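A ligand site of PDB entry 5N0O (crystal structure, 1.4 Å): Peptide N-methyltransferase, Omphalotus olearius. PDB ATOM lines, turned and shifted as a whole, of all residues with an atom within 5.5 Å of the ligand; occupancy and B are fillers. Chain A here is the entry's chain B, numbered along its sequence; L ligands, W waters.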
ATOM      1  N   ILE A  18       8.362 -10.970 -27.365  1.00  0.00           N
ATOM      2  CA  ILE A  18       8.323 -12.134 -26.436  1.00  0.00           C
ATOM      3  C   ILE A  18       9.711 -12.411 -25.816  1.00  0.00           C
ATOM      4  O   ILE A  18       9.839 -12.547 -24.594  1.00  0.00           O
ATOM      5  CB  ILE A  18       7.756 -13.401 -27.138  1.00  0.00           C
ATOM      6  CG1 ILE A  18       6.306 -13.158 -27.609  1.00  0.00           C
ATOM      7  CG2 ILE A  18       7.843 -14.632 -26.239  1.00  0.00           C
ATOM      8  CD1 ILE A  18       5.282 -12.978 -26.485  1.00  0.00           C
ATOM      9  N   ILE A  43       6.560  -9.919 -18.186  1.00  0.00           N
ATOM     10  CA  ILE A  43       6.693 -11.137 -17.368  1.00  0.00           C
ATOM     11  C   ILE A  43       8.107 -11.708 -17.288  1.00  0.00           C
ATOM     12  O   ILE A  43       8.262 -12.910 -16.980  1.00  0.00           O
ATOM     13  CB  ILE A  43       5.646 -12.205 -17.766  1.00  0.00           C
ATOM     14  CG1 ILE A  43       5.748 -12.571 -19.247  1.00  0.00           C
ATOM     15  CG2 ILE A  43       4.245 -11.704 -17.444  1.00  0.00           C
ATOM     16  CD1 ILE A  43       5.043 -13.877 -19.585  1.00  0.00           C
ATOM     17  N   TYR A  97       3.732  -6.939 -22.753  1.00  0.00           N
ATOM     18  CA  TYR A  97       4.627  -7.868 -23.467  1.00  0.00           C
ATOM     19  C   TYR A  97       3.980  -8.440 -24.747  1.00  0.00           C
ATOM     20  O   TYR A  97       2.749  -8.497 -24.870  1.00  0.00           O
ATOM     21  CB  TYR A  97       5.167  -8.962 -22.548  1.00  0.00           C
ATOM     22  CG  TYR A  97       4.244 -10.130 -22.287  1.00  0.00           C
ATOM     23  CD1 TYR A  97       3.349 -10.127 -21.212  1.00  0.00           C
ATOM     24  CD2 TYR A  97       4.298 -11.269 -23.088  1.00  0.00           C
ATOM     25  CE1 TYR A  97       2.508 -11.225 -20.984  1.00  0.00           C
ATOM     26  CE2 TYR A  97       3.467 -12.354 -22.867  1.00  0.00           C
ATOM     27  CZ  TYR A  97       2.578 -12.336 -21.816  1.00  0.00           C
ATOM     28  OH  TYR A  97       1.761 -13.439 -21.594  1.00  0.00           O
ATOM     29  N   GLY A  98       4.828  -8.769 -25.721  1.00  0.00           N
ATOM     30  CA  GLY A  98       4.379  -9.236 -27.047  1.00  0.00           C
ATOM     31  C   GLY A  98       3.847  -8.102 -27.900  1.00  0.00           C
ATOM     32  O   GLY A  98       4.490  -7.033 -27.987  1.00  0.00           O
ATOM     33  N   HIS A  99       2.691  -8.320 -28.542  1.00  0.00           N
ATOM     34  CA  HIS A  99       1.871  -7.298 -29.214  1.00  0.00           C
ATOM     35  C   HIS A  99       0.823  -6.851 -28.189  1.00  0.00           C
ATOM     36  O   HIS A  99       0.129  -7.706 -27.596  1.00  0.00           O
ATOM     37  CB  HIS A  99       1.223  -7.914 -30.461  1.00  0.00           C
ATOM     38  CG  HIS A  99       0.383  -6.985 -31.308  1.00  0.00           C
ATOM     39  ND1 HIS A  99      -0.626  -6.186 -30.802  1.00  0.00           N
ATOM     40  CD2 HIS A  99       0.359  -6.802 -32.647  1.00  0.00           C
ATOM     41  CE1 HIS A  99      -1.222  -5.548 -31.808  1.00  0.00           C
ATOM     42  NE2 HIS A  99      -0.642  -5.905 -32.939  1.00  0.00           N
ATOM     43  N   PRO A 100       0.709  -5.535 -27.938  1.00  0.00           N
ATOM     44  CA  PRO A 100      -0.125  -5.068 -26.814  1.00  0.00           C
ATOM     45  C   PRO A 100      -1.645  -5.165 -27.031  1.00  0.00           C
ATOM     46  O   PRO A 100      -2.409  -4.823 -26.106  1.00  0.00           O
ATOM     47  CB  PRO A 100       0.320  -3.611 -26.652  1.00  0.00           C
ATOM     48  CG  PRO A 100       0.673  -3.200 -28.035  1.00  0.00           C
ATOM     49  CD  PRO A 100       1.345  -4.390 -28.649  1.00  0.00           C
ATOM     50  N   VAL A 102      -2.966  -8.195 -28.730  1.00  0.00           N
ATOM     51  CA  VAL A 102      -3.191  -9.604 -29.109  1.00  0.00           C
ATOM     52  C   VAL A 102      -3.383 -10.392 -27.811  1.00  0.00           C
ATOM     53  O   VAL A 102      -2.424 -10.592 -27.063  1.00  0.00           O
ATOM     54  CB  VAL A 102      -2.022 -10.116 -29.996  1.00  0.00           C
ATOM     55  CG1 VAL A 102      -2.028 -11.634 -30.173  1.00  0.00           C
ATOM     56  CG2 VAL A 102      -2.073  -9.436 -31.350  1.00  0.00           C
ATOM     57  N   PHE A 103      -4.625 -10.817 -27.560  1.00  0.00           N
ATOM     58  CA  PHE A 103      -5.035 -11.444 -26.299  1.00  0.00           C
ATOM     59  C   PHE A 103      -4.679 -10.566 -25.087  1.00  0.00           C
ATOM     60  O   PHE A 103      -4.127 -11.043 -24.089  1.00  0.00           O
ATOM     61  CB  PHE A 103      -4.465 -12.884 -26.199  1.00  0.00           C
ATOM     62  CG  PHE A 103      -4.973 -13.814 -27.283  1.00  0.00           C
ATOM     63  CD1 PHE A 103      -4.408 -13.781 -28.549  1.00  0.00           C
ATOM     64  CD2 PHE A 103      -6.007 -14.721 -27.035  1.00  0.00           C
ATOM     65  CE1 PHE A 103      -4.865 -14.601 -29.565  1.00  0.00           C
ATOM     66  CE2 PHE A 103      -6.464 -15.541 -28.052  1.00  0.00           C
ATOM     67  CZ  PHE A 103      -5.893 -15.481 -29.317  1.00  0.00           C
ATOM     68  N   VAL A 104      -5.013  -9.275 -25.190  1.00  0.00           N
ATOM     69  CA  VAL A 104      -4.829  -8.308 -24.096  1.00  0.00           C
ATOM     70  C   VAL A 104      -6.104  -7.474 -23.952  1.00  0.00           C
ATOM     71  O   VAL A 104      -6.478  -6.754 -24.861  1.00  0.00           O
ATOM     72  CB  VAL A 104      -3.641  -7.331 -24.328  1.00  0.00           C
ATOM     73  CG1 VAL A 104      -3.487  -6.353 -23.143  1.00  0.00           C
ATOM     74  CG2 VAL A 104      -2.338  -8.096 -24.551  1.00  0.00           C
ATOM     75  N   VAL A 127       5.674  -7.755 -31.782  1.00  0.00           N
ATOM     76  CA  VAL A 127       5.872  -9.173 -32.132  1.00  0.00           C
ATOM     77  C   VAL A 127       5.097 -10.051 -31.129  1.00  0.00           C
ATOM     78  O   VAL A 127       5.420 -10.060 -29.933  1.00  0.00           O
ATOM     79  CB  VAL A 127       7.380  -9.523 -32.136  1.00  0.00           C
ATOM     80  CG1 VAL A 127       7.604 -11.029 -32.332  1.00  0.00           C
ATOM     81  CG2 VAL A 127       8.118  -8.708 -33.200  1.00  0.00           C
ATOM     82  N   SER A 128       4.095 -10.795 -31.603  1.00  0.00           N
ATOM     83  CA  SER A 128       3.251 -11.648 -30.742  1.00  0.00           C
ATOM     84  C   SER A 128       3.796 -13.069 -30.587  1.00  0.00           C
ATOM     85  O   SER A 128       4.714 -13.491 -31.317  1.00  0.00           O
ATOM     86  CB  SER A 128       1.832 -11.741 -31.335  1.00  0.00           C
ATOM     87  OG  SER A 128       1.787 -12.671 -32.435  1.00  0.00           O
ATOM     88  N   ALA A 129       3.190 -13.835 -29.682  1.00  0.00           N
ATOM     89  CA  ALA A 129       3.558 -15.264 -29.544  1.00  0.00           C
ATOM     90  C   ALA A 129       3.240 -16.069 -30.813  1.00  0.00           C
ATOM     91  O   ALA A 129       3.937 -17.048 -31.108  1.00  0.00           O
ATOM     92  CB  ALA A 129       2.876 -15.885 -28.329  1.00  0.00           C
ATOM     93  N   GLU A 130       2.222 -15.647 -31.578  1.00  0.00           N
ATOM     94  CA  GLU A 130       1.902 -16.300 -32.859  1.00  0.00           C
ATOM     95  C   GLU A 130       2.970 -16.000 -33.911  1.00  0.00           C
ATOM     96  O   GLU A 130       3.336 -16.885 -34.697  1.00  0.00           O
ATOM     97  CB  GLU A 130       0.505 -15.924 -33.357  1.00  0.00           C
ATOM     98  CG  GLU A 130       0.143 -16.647 -34.663  1.00  0.00           C
ATOM     99  CD  GLU A 130      -1.314 -16.527 -35.082  1.00  0.00           C
ATOM    100  OE1 GLU A 130      -1.695 -15.573 -35.782  1.00  0.00           O
ATOM    101  OE2 GLU A 130      -2.093 -17.452 -34.749  1.00  0.00           O
ATOM    102  N   LEU A 169      -4.140 -22.253 -30.794  1.00  0.00           N
ATOM    103  CA  LEU A 169      -4.941 -22.035 -29.566  1.00  0.00           C
ATOM    104  C   LEU A 169      -4.096 -21.384 -28.447  1.00  0.00           C
ATOM    105  O   LEU A 169      -3.123 -21.991 -27.983  1.00  0.00           O
ATOM    106  CB  LEU A 169      -5.547 -23.361 -29.054  1.00  0.00           C
ATOM    107  CG  LEU A 169      -6.468 -24.168 -29.963  1.00  0.00           C
ATOM    108  CD1 LEU A 169      -6.864 -25.497 -29.300  1.00  0.00           C
ATOM    109  CD2 LEU A 169      -7.708 -23.393 -30.362  1.00  0.00           C
ATOM    110  N   PHE A 170      -4.483 -20.174 -28.043  1.00  0.00           N
ATOM    111  CA  PHE A 170      -3.858 -19.457 -26.908  1.00  0.00           C
ATOM    112  C   PHE A 170      -4.555 -19.847 -25.595  1.00  0.00           C
ATOM    113  O   PHE A 170      -5.724 -20.265 -25.600  1.00  0.00           O
ATOM    114  CB  PHE A 170      -3.987 -17.918 -27.071  1.00  0.00           C
ATOM    115  CG  PHE A 170      -2.977 -17.277 -28.012  1.00  0.00           C
ATOM    116  CD1 PHE A 170      -2.940 -17.575 -29.360  1.00  0.00           C
ATOM    117  CD2 PHE A 170      -2.125 -16.279 -27.530  1.00  0.00           C
ATOM    118  CE1 PHE A 170      -2.044 -16.928 -30.213  1.00  0.00           C
ATOM    119  CE2 PHE A 170      -1.222 -15.626 -28.379  1.00  0.00           C
ATOM    120  CZ  PHE A 170      -1.191 -15.952 -29.727  1.00  0.00           C
ATOM    121  N   GLN A 171      -3.855 -19.671 -24.477  1.00  0.00           N
ATOM    122  CA  GLN A 171      -4.441 -19.788 -23.123  1.00  0.00           C
ATOM    123  C   GLN A 171      -4.989 -21.186 -22.815  1.00  0.00           C
ATOM    124  O   GLN A 171      -5.975 -21.357 -22.095  1.00  0.00           O
ATOM    125  CB  GLN A 171      -5.456 -18.656 -22.882  1.00  0.00           C
ATOM    126  CG  GLN A 171      -4.785 -17.282 -22.978  1.00  0.00           C
ATOM    127  CD  GLN A 171      -5.597 -16.081 -22.537  1.00  0.00           C
ATOM    128  OE1 GLN A 171      -6.797 -16.162 -22.235  1.00  0.00           O
ATOM    129  NE2 GLN A 171      -4.934 -14.933 -22.474  1.00  0.00           N
ATOM    130  N   VAL A 172      -4.281 -22.183 -23.334  1.00  0.00           N
ATOM    131  CA  VAL A 172      -4.584 -23.600 -23.093  1.00  0.00           C
ATOM    132  C   VAL A 172      -4.257 -24.014 -21.649  1.00  0.00           C
ATOM    133  O   VAL A 172      -4.752 -25.051 -21.177  1.00  0.00           O
ATOM    134  CB  VAL A 172      -3.872 -24.527 -24.120  1.00  0.00           C
ATOM    135  CG1 VAL A 172      -4.405 -24.289 -25.528  1.00  0.00           C
ATOM    136  CG2 VAL A 172      -2.350 -24.398 -24.092  1.00  0.00           C
ATOM    137  N   CSO A 174      -5.214 -22.307 -18.913  1.00  0.00           N
ATOM    138  CA  CSO A 174      -6.205 -21.761 -17.960  1.00  0.00           C
ATOM    139  CB  CSO A 174      -5.879 -20.306 -17.609  1.00  0.00           C
ATOM    140  SG  CSO A 174      -5.752 -19.257 -19.026  1.00  0.00           S
ATOM    141  C   CSO A 174      -7.627 -21.914 -18.455  1.00  0.00           C
ATOM    142  O   CSO A 174      -8.411 -20.968 -18.439  1.00  0.00           O
ATOM    143  OD  CSO A 174      -4.031 -19.357 -19.229  1.00  0.00           O
ATOM    144  N   TYR A 210       3.898 -25.593 -27.753  1.00  0.00           N
ATOM    145  CA  TYR A 210       4.849 -24.522 -28.081  1.00  0.00           C
ATOM    146  C   TYR A 210       5.039 -23.507 -26.950  1.00  0.00           C
ATOM    147  O   TYR A 210       4.067 -22.916 -26.474  1.00  0.00           O
ATOM    148  CB  TYR A 210       4.392 -23.790 -29.352  1.00  0.00           C
ATOM    149  CG  TYR A 210       5.324 -22.635 -29.735  1.00  0.00           C
ATOM    150  CD1 TYR A 210       6.654 -22.875 -30.104  1.00  0.00           C
ATOM    151  CD2 TYR A 210       4.891 -21.306 -29.704  1.00  0.00           C
ATOM    152  CE1 TYR A 210       7.512 -21.828 -30.442  1.00  0.00           C
ATOM    153  CE2 TYR A 210       5.736 -20.264 -30.038  1.00  0.00           C
ATOM    154  CZ  TYR A 210       7.054 -20.524 -30.388  1.00  0.00           C
ATOM    155  OH  TYR A 210       7.904 -19.490 -30.743  1.00  0.00           O
ATOM    156  N   ILE A 211       6.294 -23.318 -26.536  1.00  0.00           N
ATOM    157  CA  ILE A 211       6.703 -22.196 -25.670  1.00  0.00           C
ATOM    158  C   ILE A 211       7.913 -21.503 -26.304  1.00  0.00           C
ATOM    159  O   ILE A 211       9.008 -22.071 -26.349  1.00  0.00           O
ATOM    160  CB  ILE A 211       7.034 -22.618 -24.221  1.00  0.00           C
ATOM    161  CG1 ILE A 211       5.902 -23.457 -23.605  1.00  0.00           C
ATOM    162  CG2 ILE A 211       7.332 -21.379 -23.361  1.00  0.00           C
ATOM    163  CD1 ILE A 211       6.227 -24.077 -22.265  1.00  0.00           C
ATOM    164  N   ALA A 212       7.713 -20.274 -26.771  1.00  0.00           N
ATOM    165  CA  ALA A 212       8.802 -19.464 -27.314  1.00  0.00           C
ATOM    166  C   ALA A 212       9.834 -19.182 -26.220  1.00  0.00           C
ATOM    167  O   ALA A 212       9.453 -18.917 -25.066  1.00  0.00           O
ATOM    168  CB  ALA A 212       8.273 -18.151 -27.862  1.00  0.00           C
ATOM    169  N   ALA A 213      11.119 -19.204 -26.580  1.00  0.00           N
ATOM    170  CA  ALA A 213      12.196 -18.804 -25.649  1.00  0.00           C
ATOM    171  C   ALA A 213      12.000 -17.369 -25.156  1.00  0.00           C
ATOM    172  O   ALA A 213      11.799 -16.449 -25.961  1.00  0.00           O
ATOM    173  CB  ALA A 213      13.559 -18.935 -26.322  1.00  0.00           C
ATOM    174  N   MET A 214      12.066 -17.185 -23.836  1.00  0.00           N
ATOM    175  CA  MET A 214      11.941 -15.869 -23.213  1.00  0.00           C
ATOM    176  C   MET A 214      13.275 -15.193 -23.014  1.00  0.00           C
ATOM    177  O   MET A 214      13.352 -13.965 -23.090  1.00  0.00           O
ATOM    178  CB  MET A 214      11.244 -15.956 -21.866  1.00  0.00           C
ATOM    179  CG  MET A 214      10.591 -14.618 -21.560  1.00  0.00           C
ATOM    180  SD  MET A 214       9.890 -14.644 -19.737  1.00  0.00           S
ATOM    181  CE  MET A 214       8.200 -15.530 -20.192  1.00  0.00           C
ATOM    182  N   GLY A 240       1.340 -24.741 -19.144  1.00  0.00           N
ATOM    183  CA  GLY A 240       1.246 -23.635 -18.187  1.00  0.00           C
ATOM    184  C   GLY A 240       0.777 -22.318 -18.803  1.00  0.00           C
ATOM    185  O   GLY A 240       0.198 -22.302 -19.900  1.00  0.00           O
ATOM    186  N   GLY A 241       1.043 -21.221 -18.106  1.00  0.00           N
ATOM    187  CA  GLY A 241       0.525 -19.914 -18.473  1.00  0.00           C
ATOM    188  C   GLY A 241       1.138 -19.251 -19.685  1.00  0.00           C
ATOM    189  O   GLY A 241       0.597 -18.255 -20.171  1.00  0.00           O
ATOM    190  N   VAL A 242       2.280 -19.767 -20.173  1.00  0.00           N
ATOM    191  CA  VAL A 242       2.909 -19.272 -21.414  1.00  0.00           C
ATOM    192  C   VAL A 242       2.915 -20.335 -22.531  1.00  0.00           C
ATOM    193  O   VAL A 242       3.692 -20.252 -23.481  1.00  0.00           O
ATOM    194  CB  VAL A 242       4.333 -18.681 -21.154  1.00  0.00           C
ATOM    195  CG1 VAL A 242       4.232 -17.426 -20.303  1.00  0.00           C
ATOM    196  CG2 VAL A 242       5.284 -19.691 -20.530  1.00  0.00           C
ATOM    197  N   SER A 243       2.026 -21.326 -22.425  1.00  0.00           N
ATOM    198  CA  SER A 243       1.883 -22.397 -23.430  1.00  0.00           C
ATOM    199  C   SER A 243       0.836 -22.077 -24.493  1.00  0.00           C
ATOM    200  O   SER A 243      -0.255 -21.596 -24.181  1.00  0.00           O
ATOM    201  CB  SER A 243       1.477 -23.703 -22.738  1.00  0.00           C
ATOM    202  OG  SER A 243       2.488 -24.198 -21.876  1.00  0.00           O
ATOM    203  N   THR A 244       1.165 -22.387 -25.751  1.00  0.00           N
ATOM    204  CA  THR A 244       0.259 -22.260 -26.904  1.00  0.00           C
ATOM    205  C   THR A 244       0.251 -23.611 -27.634  1.00  0.00           C
ATOM    206  O   THR A 244       1.275 -24.288 -27.658  1.00  0.00           O
ATOM    207  CB  THR A 244       0.718 -21.088 -27.821  1.00  0.00           C
ATOM    208  OG1 THR A 244       0.619 -19.837 -27.114  1.00  0.00           O
ATOM    209  CG2 THR A 244      -0.085 -20.993 -29.120  1.00  0.00           C
HETATM  210  N1  LIG L   1       0.148 -10.143 -25.865  1.00  0.00           N
HETATM  211  C1  LIG L   1       0.708 -11.499 -25.852  1.00  0.00           C
HETATM  212  C2  LIG L   1       1.221 -11.814 -27.256  1.00  0.00           C
HETATM  213  O1  LIG L   1       1.405 -10.863 -28.069  1.00  0.00           O
HETATM  214  O2  LIG L   1       1.461 -13.003 -27.563  1.00  0.00           O
HETATM  215  C3  LIG L   1      -0.330 -12.557 -25.334  1.00  0.00           C
HETATM  216  C4  LIG L   1      -0.969 -12.340 -23.931  1.00  0.00           C
HETATM  217  S1  LIG L   1      -2.054 -13.485 -23.283  1.00  0.00           S
HETATM  218  C5  LIG L   1      -2.624 -12.806 -21.862  1.00  0.00           C
HETATM  219  C6  LIG L   1      -1.239 -14.884 -22.757  1.00  0.00           C
HETATM  220  C7  LIG L   1      -1.132 -16.080 -23.730  1.00  0.00           C
HETATM  221  O3  LIG L   1      -0.138 -15.795 -24.723  1.00  0.00           O
HETATM  222  C8  LIG L   1      -0.634 -17.416 -23.152  1.00  0.00           C
HETATM  223  O4  LIG L   1      -1.656 -18.205 -22.517  1.00  0.00           O
HETATM  224  C9  LIG L   1      -0.047 -18.118 -24.359  1.00  0.00           C
HETATM  225  O5  LIG L   1      -1.064 -18.742 -25.166  1.00  0.00           O
HETATM  226  C10 LIG L   1       0.585 -16.957 -25.128  1.00  0.00           C
HETATM  227  N2  LIG L   1       2.029 -16.834 -24.795  1.00  0.00           N
HETATM  228  C11 LIG L   1       2.612 -15.920 -23.962  1.00  0.00           C
HETATM  229  N3  LIG L   1       3.951 -16.108 -23.883  1.00  0.00           N
HETATM  230  C12 LIG L   1       4.234 -17.171 -24.674  1.00  0.00           C
HETATM  231  C13 LIG L   1       5.455 -17.901 -25.036  1.00  0.00           C
HETATM  232  N4  LIG L   1       6.654 -17.538 -24.524  1.00  0.00           N
HETATM  233  N5  LIG L   1       5.326 -18.929 -25.903  1.00  0.00           N
HETATM  234  C14 LIG L   1       4.128 -19.292 -26.415  1.00  0.00           C
HETATM  235  N6  LIG L   1       2.971 -18.681 -26.125  1.00  0.00           N
HETATM  236  C15 LIG L   1       2.978 -17.621 -25.273  1.00  0.00           C
HETATM  237  O   HOH W   1       0.590  -9.036 -23.269  1.00  0.00           O
HETATM  238  O   HOH W   2      -1.438 -21.033 -21.786  1.00  0.00           O
HETATM  239  O   HOH W   3       6.325 -15.060 -22.795  1.00  0.00           O
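OG1 of Thr 244 sits at hydrogen-bond distance from O5 of the ligand. An oxygen (O2) of the ligand sits at hydrogen-bond distance from the backbone NH (N) of Ala 129. A nitrogen (N1) of the ligand is in hydrogen-bond range of the backbone carbonyl oxygen of Val 102, at 2.9 Å. N of Ala 212 lies within hydrogen-bond range of N5 of the ligand (2.9 Å). The backbone carbonyl oxygen (O) of Ala 212 is in hydrogen-bond range of a nitrogen (N4) of the ligand (3.2 Å). The backbone NH (N) of His 99 sits at hydrogen-bond distance from an oxygen (O1) of the ligand (2.9 Å). N1 of the ligand sits at hydrogen-bond distance from O of His 99 (3.0 Å). O5 of the ligand is in hydrogen-bond range of N of Gln 171, at 3.0 Å. O of Ser 243 lies within hydrogen-bond range of O5 of the ligand (3.1 Å). A nitrogen (N1) of the ligand lies within hydrogen-bond range of the backbone carbonyl oxygen (O) of Tyr 97, at 3.2 Å. The backbone carbonyl oxygen of Gly 241 lies within hydrogen-bond range of an oxygen (O4) of the ligand, 3.3 Å away.
The backbone carbonyl oxygen of Thr 244 is in hydrogen-bond range of the backbone NH of Tyr 210. N of Gly 240 lies within hydrogen-bond range of OG of Ser 243 (3.0 Å). The side-chain hydroxyl (OG) of Ser 128 is in hydrogen-bond range of the backbone NH (N) of Glu 130 (3.1 Å).
Water W1 bridges O of Tyr 97 (2.7 Å) and N1 of the ligand (2.9 Å). Water W2 lies within hydrogen-bond range of O of Ser 243 (2.7 Å), O of Gly 240 (2.8 Å), O4 of the ligand (2.9 Å) and N of Val 172 (3.4 Å).
A sulfur (S1) of the ligand lies close to the backbone carbonyl oxygen (O) of Phe 103, at 3.3 Å. O of Val 242 sits close to N6 of the ligand (3.2 Å). Ile 18 touches the ligand. Gly 98 touches the ligand. Val 104 touches the ligand. Ser 128 touches the ligand. Phe 170 touches the ligand (CA to O5, 3.4 Å). Tyr 210 touches the ligand (O to C14, 3.6 Å). Ile 211 touches the ligand (CA to N5, 3.6 Å). Hydrophobic or aromatic side chains within 4 Å of the ligand: Ile 18, Tyr 97, His 99, Phe 103, Val 104, Ala 129, Phe 170, Tyr 210, Ala 212 and Val 242. The nearest printed residue that does not touch the ligand is CSO 174 (4.2 Å).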
